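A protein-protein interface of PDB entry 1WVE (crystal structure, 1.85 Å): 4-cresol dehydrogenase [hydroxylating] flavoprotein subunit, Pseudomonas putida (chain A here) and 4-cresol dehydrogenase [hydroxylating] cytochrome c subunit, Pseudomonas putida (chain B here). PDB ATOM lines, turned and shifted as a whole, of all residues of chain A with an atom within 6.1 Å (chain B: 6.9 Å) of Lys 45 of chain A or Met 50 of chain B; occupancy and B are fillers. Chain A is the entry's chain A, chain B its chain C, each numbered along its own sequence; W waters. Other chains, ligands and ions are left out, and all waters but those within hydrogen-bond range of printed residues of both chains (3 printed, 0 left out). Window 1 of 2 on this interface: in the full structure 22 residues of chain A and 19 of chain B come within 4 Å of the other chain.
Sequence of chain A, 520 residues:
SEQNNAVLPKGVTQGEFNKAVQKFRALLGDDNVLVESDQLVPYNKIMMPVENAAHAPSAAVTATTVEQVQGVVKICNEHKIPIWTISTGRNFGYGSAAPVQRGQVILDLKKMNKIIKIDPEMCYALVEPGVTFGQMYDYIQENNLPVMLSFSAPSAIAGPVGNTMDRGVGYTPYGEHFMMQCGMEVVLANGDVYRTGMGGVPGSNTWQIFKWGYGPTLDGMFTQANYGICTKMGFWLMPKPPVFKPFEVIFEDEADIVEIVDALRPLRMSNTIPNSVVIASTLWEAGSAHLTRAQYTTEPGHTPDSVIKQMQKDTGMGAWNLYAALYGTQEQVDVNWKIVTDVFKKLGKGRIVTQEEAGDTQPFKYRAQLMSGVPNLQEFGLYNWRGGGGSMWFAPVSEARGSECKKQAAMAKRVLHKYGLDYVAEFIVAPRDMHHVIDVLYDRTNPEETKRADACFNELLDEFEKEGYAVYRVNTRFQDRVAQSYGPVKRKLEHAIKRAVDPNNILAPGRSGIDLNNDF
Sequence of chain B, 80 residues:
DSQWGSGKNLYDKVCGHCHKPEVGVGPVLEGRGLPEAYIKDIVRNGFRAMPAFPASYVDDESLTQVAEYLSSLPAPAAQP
Water W1 lies within hydrogen-bond range of O of Val 41 of chain A (2.6 Å), O of Asn 45 of chain B (2.9 Å) and N of Lys 45 of chain A (3.4 Å). Water W3 lies within hydrogen-bond range of the backbone carbonyl oxygen (O) of Ala 49 of chain B (2.7 Å) and the side-chain sulfur (SD) of Met 47 of chain A (3.5 Å). Water W2 bridges the backbone carbonyl oxygen of Pro 42 of chain A (2.8 Å) and the backbone carbonyl oxygen of Ala 52 of chain B (3.5 Å).
The side-chain amino group (NZ) of Lys 45 of chain A lies within hydrogen-bond range of the backbone carbonyl oxygen (O) of Arg 48 of chain B (2.7 Å). The side-chain amino group of Lys 45 of chain A sits close to the backbone carbonyl oxygen of Met 50 of chain B (3.5 Å). The backbone nitrogen (N) of Pro 42 of chain A lies close to the backbone carbonyl oxygen (O) of Arg 44 of chain B (3.2 Å).
The backbone NH (N) of Phe 53 of chain B is in hydrogen-bond range of the backbone carbonyl oxygen (O) of Val 43 of chain B (2.9 Å). The backbone carbonyl oxygen (O) of Phe 53 of chain B sits at hydrogen-bond distance from the guanidinium group (NH1) of Arg 44 of chain B, 2.9 Å away.
Hydrophobic or aromatic side chains of chain A that line the printed part of chain B: Val 41 and Pro 42. Of the 14 printed residues of chain B, 9 touch a printed residue of chain A. Hydrophobic or aromatic side chains of chain B that line the printed part of chain A: Ala 52. Among the printed residues, no Asp or Glu carboxylate lies within 4 Å of a Lys or Arg side-chain nitrogen of the other chain.
Val 41 of chain A touches Arg 44 of chain B. CG2 of Val 41 of chain A touches OD1 of Asn 45 of chain B, 3.3 Å away. Pro 42 of chain A touches Ala 52 of chain B. Pro 42 of chain A touches Phe 53 of chain B. Lys 45 of chain A touches Asn 45 of chain B. Lys 45 of chain A touches Gly 46 of chain B (CE to C, 3.8 Å). Lys 45 of chain A touches Phe 47 of chain B (CE to N, 3.6 Å). CB of Lys 45 of chain A touches CB of Ala 52 of chain B, 3.6 Å away. CA of Gly 389 of chain A touches O of Arg 48 of chain B (3.4 Å). Ala 49 of chain B touches Gly 389 of chain A (N to N, 3.8 Å).
Lys 45 of chain A touches just these residues of chain B: Asn 45, Gly 46, Phe 47, Arg 48, Met 50 and Ala 52. Met 50 of chain B touches one residue of chain A. Printed residues of chain A within 4 Å of Gly 46 of chain B: Lys 45. Of the printed residues of chain A, Arg 48 of chain B touches Lys 45 (2.7 Å) and Gly 389 (3.4 Å). Printed residues of chain A within 4 Å of Phe 53 of chain B: Pro 42. The nearest residue of chain A that does not touch Met 50 of chain B is Gly 389 of chain A (6.0 Å).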
ATOM      1  N   LEU A  40      27.114  -5.443 -10.243  1.00  0.00           N
ATOM      2  CA  LEU A  40      26.385  -5.191  -9.014  1.00  0.00           C
ATOM      3  C   LEU A  40      25.270  -4.143  -9.073  1.00  0.00           C
ATOM      4  O   LEU A  40      24.338  -4.190  -8.268  1.00  0.00           O
ATOM      5  CB  LEU A  40      27.387  -4.807  -7.917  1.00  0.00           C
ATOM      6  CG  LEU A  40      28.440  -5.880  -7.608  1.00  0.00           C
ATOM      7  CD1 LEU A  40      29.436  -5.352  -6.559  1.00  0.00           C
ATOM      8  CD2 LEU A  40      27.733  -7.155  -7.113  1.00  0.00           C
ATOM      9  N   VAL A  41      25.357  -3.210 -10.020  1.00  0.00           N
ATOM     10  CA  VAL A  41      24.359  -2.146 -10.117  1.00  0.00           C
ATOM     11  C   VAL A  41      22.895  -2.623 -10.159  1.00  0.00           C
ATOM     12  O   VAL A  41      22.029  -1.987  -9.563  1.00  0.00           O
ATOM     13  CB  VAL A  41      24.670  -1.185 -11.313  1.00  0.00           C
ATOM     14  CG1 VAL A  41      24.427  -1.871 -12.650  1.00  0.00           C
ATOM     15  CG2 VAL A  41      23.843   0.077 -11.181  1.00  0.00           C
ATOM     16  N   PRO A  42      22.595  -3.742 -10.852  1.00  0.00           N
ATOM     17  CA  PRO A  42      21.186  -4.147 -10.841  1.00  0.00           C
ATOM     18  C   PRO A  42      20.643  -4.514  -9.454  1.00  0.00           C
ATOM     19  O   PRO A  42      19.450  -4.364  -9.206  1.00  0.00           O
ATOM     20  CB  PRO A  42      21.143  -5.316 -11.824  1.00  0.00           C
ATOM     21  CG  PRO A  42      22.542  -5.813 -11.872  1.00  0.00           C
ATOM     22  CD  PRO A  42      23.376  -4.575 -11.784  1.00  0.00           C
ATOM     23  N   TYR A  43      21.512  -5.011  -8.572  1.00  0.00           N
ATOM     24  CA  TYR A  43      21.113  -5.389  -7.209  1.00  0.00           C
ATOM     25  C   TYR A  43      20.928  -4.140  -6.330  1.00  0.00           C
ATOM     26  O   TYR A  43      20.275  -4.184  -5.276  1.00  0.00           O
ATOM     27  CB  TYR A  43      22.203  -6.246  -6.555  1.00  0.00           C
ATOM     28  CG  TYR A  43      22.450  -7.600  -7.174  1.00  0.00           C
ATOM     29  CD1 TYR A  43      21.631  -8.686  -6.874  1.00  0.00           C
ATOM     30  CD2 TYR A  43      23.534  -7.807  -8.035  1.00  0.00           C
ATOM     31  CE1 TYR A  43      21.883  -9.949  -7.413  1.00  0.00           C
ATOM     32  CE2 TYR A  43      23.797  -9.058  -8.575  1.00  0.00           C
ATOM     33  CZ  TYR A  43      22.970 -10.126  -8.261  1.00  0.00           C
ATOM     34  OH  TYR A  43      23.232 -11.368  -8.789  1.00  0.00           O
ATOM     35  N   ASN A  44      21.528  -3.036  -6.763  1.00  0.00           N
ATOM     36  CA  ASN A  44      21.487  -1.789  -6.007  1.00  0.00           C
ATOM     37  C   ASN A  44      20.250  -0.918  -6.214  1.00  0.00           C
ATOM     38  O   ASN A  44      20.049   0.040  -5.477  1.00  0.00           O
ATOM     39  CB  ASN A  44      22.751  -0.981  -6.316  1.00  0.00           C
ATOM     40  CG  ASN A  44      23.271  -0.212  -5.108  1.00  0.00           C
ATOM     41  OD1 ASN A  44      24.479  -0.014  -4.968  1.00  0.00           O
ATOM     42  ND2 ASN A  44      22.364   0.232  -4.236  1.00  0.00           N
ATOM     43  N   LYS A  45      19.424  -1.244  -7.204  1.00  0.00           N
ATOM     44  CA  LYS A  45      18.222  -0.459  -7.488  1.00  0.00           C
ATOM     45  C   LYS A  45      17.249  -0.466  -6.300  1.00  0.00           C
ATOM     46  O   LYS A  45      16.717  -1.515  -5.936  1.00  0.00           O
ATOM     47  CB  LYS A  45      17.530  -1.002  -8.748  1.00  0.00           C
ATOM     48  CG  LYS A  45      16.290  -0.225  -9.253  1.00  0.00           C
ATOM     49  CD  LYS A  45      16.624   1.190  -9.724  1.00  0.00           C
ATOM     50  CE  LYS A  45      15.460   1.836 -10.494  1.00  0.00           C
ATOM     51  NZ  LYS A  45      14.198   2.097  -9.714  1.00  0.00           N
ATOM     52  N   ILE A  46      17.021   0.707  -5.702  1.00  0.00           N
ATOM     53  CA  ILE A  46      16.114   0.810  -4.554  1.00  0.00           C
ATOM     54  C   ILE A  46      15.086   1.922  -4.700  1.00  0.00           C
ATOM     55  O   ILE A  46      15.302   2.889  -5.438  1.00  0.00           O
ATOM     56  CB  ILE A  46      16.889   1.053  -3.227  1.00  0.00           C
ATOM     57  CG1 ILE A  46      17.778   2.294  -3.359  1.00  0.00           C
ATOM     58  CG2 ILE A  46      17.757  -0.161  -2.893  1.00  0.00           C
ATOM     59  CD1 ILE A  46      18.503   2.651  -2.066  1.00  0.00           C
ATOM     60  N   MET A  47      13.977   1.792  -3.972  1.00  0.00           N
ATOM     61  CA  MET A  47      12.917   2.787  -4.023  1.00  0.00           C
ATOM     62  C   MET A  47      12.842   3.559  -2.703  1.00  0.00           C
ATOM     63  O   MET A  47      11.919   4.352  -2.488  1.00  0.00           O
ATOM     64  CB  MET A  47      11.564   2.121  -4.326  1.00  0.00           C
ATOM     65  CG  MET A  47      11.554   1.271  -5.600  1.00  0.00           C
ATOM     66  SD  MET A  47       9.917   0.726  -6.135  1.00  0.00           S
ATOM     67  CE  MET A  47       9.319   2.181  -6.985  1.00  0.00           C
ATOM     68  N   ASN A  52      21.868   5.322  -3.265  1.00  0.00           N
ATOM     69  CA  ASN A  52      22.222   3.931  -3.533  1.00  0.00           C
ATOM     70  C   ASN A  52      23.362   3.412  -2.661  1.00  0.00           C
ATOM     71  O   ASN A  52      23.336   2.264  -2.196  1.00  0.00           O
ATOM     72  CB  ASN A  52      22.614   3.784  -5.008  1.00  0.00           C
ATOM     73  CG  ASN A  52      21.413   3.726  -5.926  1.00  0.00           C
ATOM     74  OD1 ASN A  52      20.281   4.013  -5.517  1.00  0.00           O
ATOM     75  ND2 ASN A  52      21.649   3.352  -7.181  1.00  0.00           N
ATOM     76  N   GLY A  95      12.955  -2.657   0.101  1.00  0.00           N
ATOM     77  CA  GLY A  95      14.396  -2.724  -0.055  1.00  0.00           C
ATOM     78  C   GLY A  95      14.868  -3.459  -1.301  1.00  0.00           C
ATOM     79  O   GLY A  95      16.069  -3.502  -1.588  1.00  0.00           O
ATOM     80  N   SER A  96      13.928  -4.033  -2.043  1.00  0.00           N
ATOM     81  CA  SER A  96      14.254  -4.765  -3.269  1.00  0.00           C
ATOM     82  C   SER A  96      15.328  -5.852  -3.077  1.00  0.00           C
ATOM     83  O   SER A  96      15.185  -6.693  -2.195  1.00  0.00           O
ATOM     84  CB  SER A  96      14.658  -3.767  -4.357  1.00  0.00           C
ATOM     85  OG  SER A  96      13.594  -2.854  -4.564  1.00  0.00           O
ATOM     86  N   ALA A  97      16.389  -5.852  -3.889  1.00  0.00           N
ATOM     87  CA  ALA A  97      17.432  -6.891  -3.760  1.00  0.00           C
ATOM     88  C   ALA A  97      18.701  -6.437  -3.042  1.00  0.00           C
ATOM     89  O   ALA A  97      19.658  -7.224  -2.870  1.00  0.00           O
ATOM     90  CB  ALA A  97      17.800  -7.446  -5.153  1.00  0.00           C
ATOM     91  N   ALA A  98      18.714  -5.180  -2.607  1.00  0.00           N
ATOM     92  CA  ALA A  98      19.883  -4.618  -1.934  1.00  0.00           C
ATOM     93  C   ALA A  98      19.971  -5.040  -0.458  1.00  0.00           C
ATOM     94  O   ALA A  98      18.945  -5.220   0.216  1.00  0.00           O
ATOM     95  CB  ALA A  98      19.872  -3.082  -2.064  1.00  0.00           C
ATOM     96  N   GLY A 389      10.475   6.697  -9.192  1.00  0.00           N
ATOM     97  CA  GLY A 389      11.089   5.586  -8.487  1.00  0.00           C
ATOM     98  C   GLY A 389      10.989   5.597  -6.971  1.00  0.00           C
ATOM     99  O   GLY A 389      11.667   4.829  -6.304  1.00  0.00           O
ATOM    100  N   ARG A 444      11.610  10.131  -6.343  1.00  0.00           N
ATOM    101  CA  ARG A 444      12.941   9.931  -5.800  1.00  0.00           C
ATOM    102  C   ARG A 444      14.025  10.696  -6.581  1.00  0.00           C
ATOM    103  O   ARG A 444      15.154  10.812  -6.112  1.00  0.00           O
ATOM    104  CB  ARG A 444      13.255   8.423  -5.739  1.00  0.00           C
ATOM    105  CG  ARG A 444      14.591   8.063  -5.088  1.00  0.00           C
ATOM    106  CD  ARG A 444      14.680   6.537  -4.795  1.00  0.00           C
ATOM    107  NE  ARG A 444      15.967   6.155  -4.217  1.00  0.00           N
ATOM    108  CZ  ARG A 444      17.090   5.982  -4.918  1.00  0.00           C
ATOM    109  NH1 ARG A 444      17.093   6.154  -6.239  1.00  0.00           N
ATOM    110  NH2 ARG A 444      18.217   5.651  -4.299  1.00  0.00           N
ATOM    111  N   HIS B  19       5.034  -3.787 -20.275  1.00  0.00           N
ATOM    112  CA  HIS B  19       5.170  -3.070 -21.541  1.00  0.00           C
ATOM    113  C   HIS B  19       4.184  -3.335 -22.689  1.00  0.00           C
ATOM    114  O   HIS B  19       4.082  -2.511 -23.600  1.00  0.00           O
ATOM    115  CB  HIS B  19       6.613  -3.241 -22.060  1.00  0.00           C
ATOM    116  CG  HIS B  19       7.621  -2.413 -21.320  1.00  0.00           C
ATOM    117  ND1 HIS B  19       7.723  -1.069 -21.548  1.00  0.00           N
ATOM    118  CD2 HIS B  19       8.419  -3.003 -20.395  1.00  0.00           C
ATOM    119  CE1 HIS B  19       8.717  -0.726 -20.659  1.00  0.00           C
ATOM    120  NE2 HIS B  19       9.160  -1.871 -19.941  1.00  0.00           N
ATOM    121  N   ILE B  39      18.601  -0.990 -24.219  1.00  0.00           N
ATOM    122  CA  ILE B  39      17.802  -1.968 -23.495  1.00  0.00           C
ATOM    123  C   ILE B  39      18.614  -2.598 -22.353  1.00  0.00           C
ATOM    124  O   ILE B  39      18.117  -2.713 -21.231  1.00  0.00           O
ATOM    125  CB  ILE B  39      17.289  -3.052 -24.459  1.00  0.00           C
ATOM    126  CG1 ILE B  39      16.228  -2.429 -25.384  1.00  0.00           C
ATOM    127  CG2 ILE B  39      16.729  -4.231 -23.679  1.00  0.00           C
ATOM    128  CD1 ILE B  39      15.755  -3.319 -26.495  1.00  0.00           C
ATOM    129  N   ILE B  42      19.021   0.000 -19.552  1.00  0.00           N
ATOM    130  CA  ILE B  42      17.784   0.210 -18.785  1.00  0.00           C
ATOM    131  C   ILE B  42      17.485  -0.976 -17.863  1.00  0.00           C
ATOM    132  O   ILE B  42      17.105  -0.792 -16.706  1.00  0.00           O
ATOM    133  CB  ILE B  42      16.565   0.429 -19.720  1.00  0.00           C
ATOM    134  CG1 ILE B  42      16.675   1.791 -20.428  1.00  0.00           C
ATOM    135  CG2 ILE B  42      15.246   0.336 -18.912  1.00  0.00           C
ATOM    136  CD1 ILE B  42      16.486   3.002 -19.508  1.00  0.00           C
ATOM    137  N   VAL B  43      17.665  -2.191 -18.372  1.00  0.00           N
ATOM    138  CA  VAL B  43      17.390  -3.383 -17.575  1.00  0.00           C
ATOM    139  C   VAL B  43      18.393  -3.568 -16.431  1.00  0.00           C
ATOM    140  O   VAL B  43      17.999  -3.909 -15.320  1.00  0.00           O
ATOM    141  CB  VAL B  43      17.371  -4.648 -18.464  1.00  0.00           C
ATOM    142  CG1 VAL B  43      17.192  -5.906 -17.610  1.00  0.00           C
ATOM    143  CG2 VAL B  43      16.210  -4.547 -19.463  1.00  0.00           C
ATOM    144  N   ARG B  44      19.676  -3.327 -16.694  1.00  0.00           N
ATOM    145  CA  ARG B  44      20.699  -3.494 -15.659  1.00  0.00           C
ATOM    146  C   ARG B  44      20.680  -2.421 -14.579  1.00  0.00           C
ATOM    147  O   ARG B  44      20.926  -2.706 -13.408  1.00  0.00           O
ATOM    148  CB  ARG B  44      22.091  -3.531 -16.285  1.00  0.00           C
ATOM    149  CG  ARG B  44      22.365  -4.782 -17.101  1.00  0.00           C
ATOM    150  CD  ARG B  44      22.454  -6.035 -16.216  1.00  0.00           C
ATOM    151  NE  ARG B  44      22.686  -7.209 -17.046  1.00  0.00           N
ATOM    152  CZ  ARG B  44      21.812  -8.188 -17.230  1.00  0.00           C
ATOM    153  NH1 ARG B  44      20.623  -8.160 -16.622  1.00  0.00           N
ATOM    154  NH2 ARG B  44      22.117  -9.175 -18.058  1.00  0.00           N
ATOM    155  N   ASN B  45      20.397  -1.184 -14.969  1.00  0.00           N
ATOM    156  CA  ASN B  45      20.373  -0.090 -13.994  1.00  0.00           C
ATOM    157  C   ASN B  45      19.005   0.132 -13.379  1.00  0.00           C
ATOM    158  O   ASN B  45      18.896   0.612 -12.244  1.00  0.00           O
ATOM    159  CB  ASN B  45      20.817   1.228 -14.650  1.00  0.00           C
ATOM    160  CG  ASN B  45      22.311   1.286 -14.890  1.00  0.00           C
ATOM    161  OD1 ASN B  45      23.082   1.558 -13.973  1.00  0.00           O
ATOM    162  ND2 ASN B  45      22.729   1.014 -16.124  1.00  0.00           N
ATOM    163  N   GLY B  46      17.967  -0.239 -14.123  1.00  0.00           N
ATOM    164  CA  GLY B  46      16.611   0.006 -13.685  1.00  0.00           C
ATOM    165  C   GLY B  46      16.393   1.443 -14.141  1.00  0.00           C
ATOM    166  O   GLY B  46      17.352   2.102 -14.551  1.00  0.00           O
ATOM    167  N   PHE B  47      15.169   1.949 -14.090  1.00  0.00           N
ATOM    168  CA  PHE B  47      14.948   3.329 -14.512  1.00  0.00           C
ATOM    169  C   PHE B  47      13.714   3.915 -13.860  1.00  0.00           C
ATOM    170  O   PHE B  47      12.591   3.656 -14.282  1.00  0.00           O
ATOM    171  CB  PHE B  47      14.825   3.428 -16.038  1.00  0.00           C
ATOM    172  CG  PHE B  47      14.674   4.840 -16.538  1.00  0.00           C
ATOM    173  CD1 PHE B  47      15.530   5.842 -16.089  1.00  0.00           C
ATOM    174  CD2 PHE B  47      13.659   5.177 -17.428  1.00  0.00           C
ATOM    175  CE1 PHE B  47      15.374   7.166 -16.514  1.00  0.00           C
ATOM    176  CE2 PHE B  47      13.496   6.496 -17.860  1.00  0.00           C
ATOM    177  CZ  PHE B  47      14.351   7.488 -17.401  1.00  0.00           C
ATOM    178  N   ARG B  48      13.941   4.705 -12.822  1.00  0.00           N
ATOM    179  CA  ARG B  48      12.860   5.332 -12.087  1.00  0.00           C
ATOM    180  C   ARG B  48      11.824   4.303 -11.661  1.00  0.00           C
ATOM    181  O   ARG B  48      12.137   3.440 -10.852  1.00  0.00           O
ATOM    182  CB  ARG B  48      12.247   6.453 -12.931  1.00  0.00           C
ATOM    183  CG  ARG B  48      13.250   7.588 -13.138  1.00  0.00           C
ATOM    184  CD  ARG B  48      12.714   8.709 -14.032  1.00  0.00           C
ATOM    185  NE  ARG B  48      13.755   9.708 -14.284  1.00  0.00           N
ATOM    186  CZ  ARG B  48      13.668  10.676 -15.196  1.00  0.00           C
ATOM    187  NH1 ARG B  48      12.581  10.784 -15.954  1.00  0.00           N
ATOM    188  NH2 ARG B  48      14.672  11.530 -15.359  1.00  0.00           N
ATOM    189  N   ALA B  49      10.607   4.366 -12.196  1.00  0.00           N
ATOM    190  CA  ALA B  49       9.571   3.409 -11.797  1.00  0.00           C
ATOM    191  C   ALA B  49       9.900   1.971 -12.191  1.00  0.00           C
ATOM    192  O   ALA B  49       9.375   1.015 -11.607  1.00  0.00           O
ATOM    193  CB  ALA B  49       8.205   3.816 -12.392  1.00  0.00           C
ATOM    194  N   MET B  50      10.752   1.808 -13.192  1.00  0.00           N
ATOM    195  CA  MET B  50      11.114   0.467 -13.628  1.00  0.00           C
ATOM    196  C   MET B  50      12.219  -0.184 -12.807  1.00  0.00           C
ATOM    197  O   MET B  50      13.277   0.400 -12.595  1.00  0.00           O
ATOM    198  CB  MET B  50      11.584   0.448 -15.073  1.00  0.00           C
ATOM    199  CG  MET B  50      11.873  -0.994 -15.528  1.00  0.00           C
ATOM    200  SD  MET B  50      12.430  -1.123 -17.221  1.00  0.00           S
ATOM    201  CE  MET B  50      13.581  -2.490 -17.067  1.00  0.00           C
ATOM    202  N   PRO B  51      11.982  -1.419 -12.356  1.00  0.00           N
ATOM    203  CA  PRO B  51      12.982  -2.145 -11.564  1.00  0.00           C
ATOM    204  C   PRO B  51      14.163  -2.610 -12.412  1.00  0.00           C
ATOM    205  O   PRO B  51      14.103  -2.618 -13.647  1.00  0.00           O
ATOM    206  CB  PRO B  51      12.193  -3.316 -10.982  1.00  0.00           C
ATOM    207  CG  PRO B  51      11.079  -3.526 -11.961  1.00  0.00           C
ATOM    208  CD  PRO B  51      10.697  -2.142 -12.411  1.00  0.00           C
ATOM    209  N   ALA B  52      15.252  -2.966 -11.745  1.00  0.00           N
ATOM    210  CA  ALA B  52      16.432  -3.468 -12.439  1.00  0.00           C
ATOM    211  C   ALA B  52      16.377  -4.981 -12.332  1.00  0.00           C
ATOM    212  O   ALA B  52      15.722  -5.517 -11.437  1.00  0.00           O
ATOM    213  CB  ALA B  52      17.688  -2.958 -11.782  1.00  0.00           C
ATOM    214  N   PHE B  53      17.053  -5.668 -13.247  1.00  0.00           N
ATOM    215  CA  PHE B  53      17.108  -7.115 -13.220  1.00  0.00           C
ATOM    216  C   PHE B  53      18.554  -7.581 -13.299  1.00  0.00           C
ATOM    217  O   PHE B  53      19.278  -7.224 -14.231  1.00  0.00           O
ATOM    218  CB  PHE B  53      16.341  -7.740 -14.401  1.00  0.00           C
ATOM    219  CG  PHE B  53      14.848  -7.639 -14.281  1.00  0.00           C
ATOM    220  CD1 PHE B  53      14.179  -6.480 -14.684  1.00  0.00           C
ATOM    221  CD2 PHE B  53      14.112  -8.684 -13.714  1.00  0.00           C
ATOM    222  CE1 PHE B  53      12.797  -6.358 -14.517  1.00  0.00           C
ATOM    223  CE2 PHE B  53      12.724  -8.572 -13.544  1.00  0.00           C
ATOM    224  CZ  PHE B  53      12.066  -7.405 -13.945  1.00  0.00           C
HETATM  225  O   HOH W   1      20.743   0.259  -9.988  1.00  0.00           O
HETATM  226  O   HOH W   2      16.982  -5.203  -8.217  1.00  0.00           O
HETATM  227  O   HOH W   3       9.983  -0.496  -9.451  1.00  0.00           O
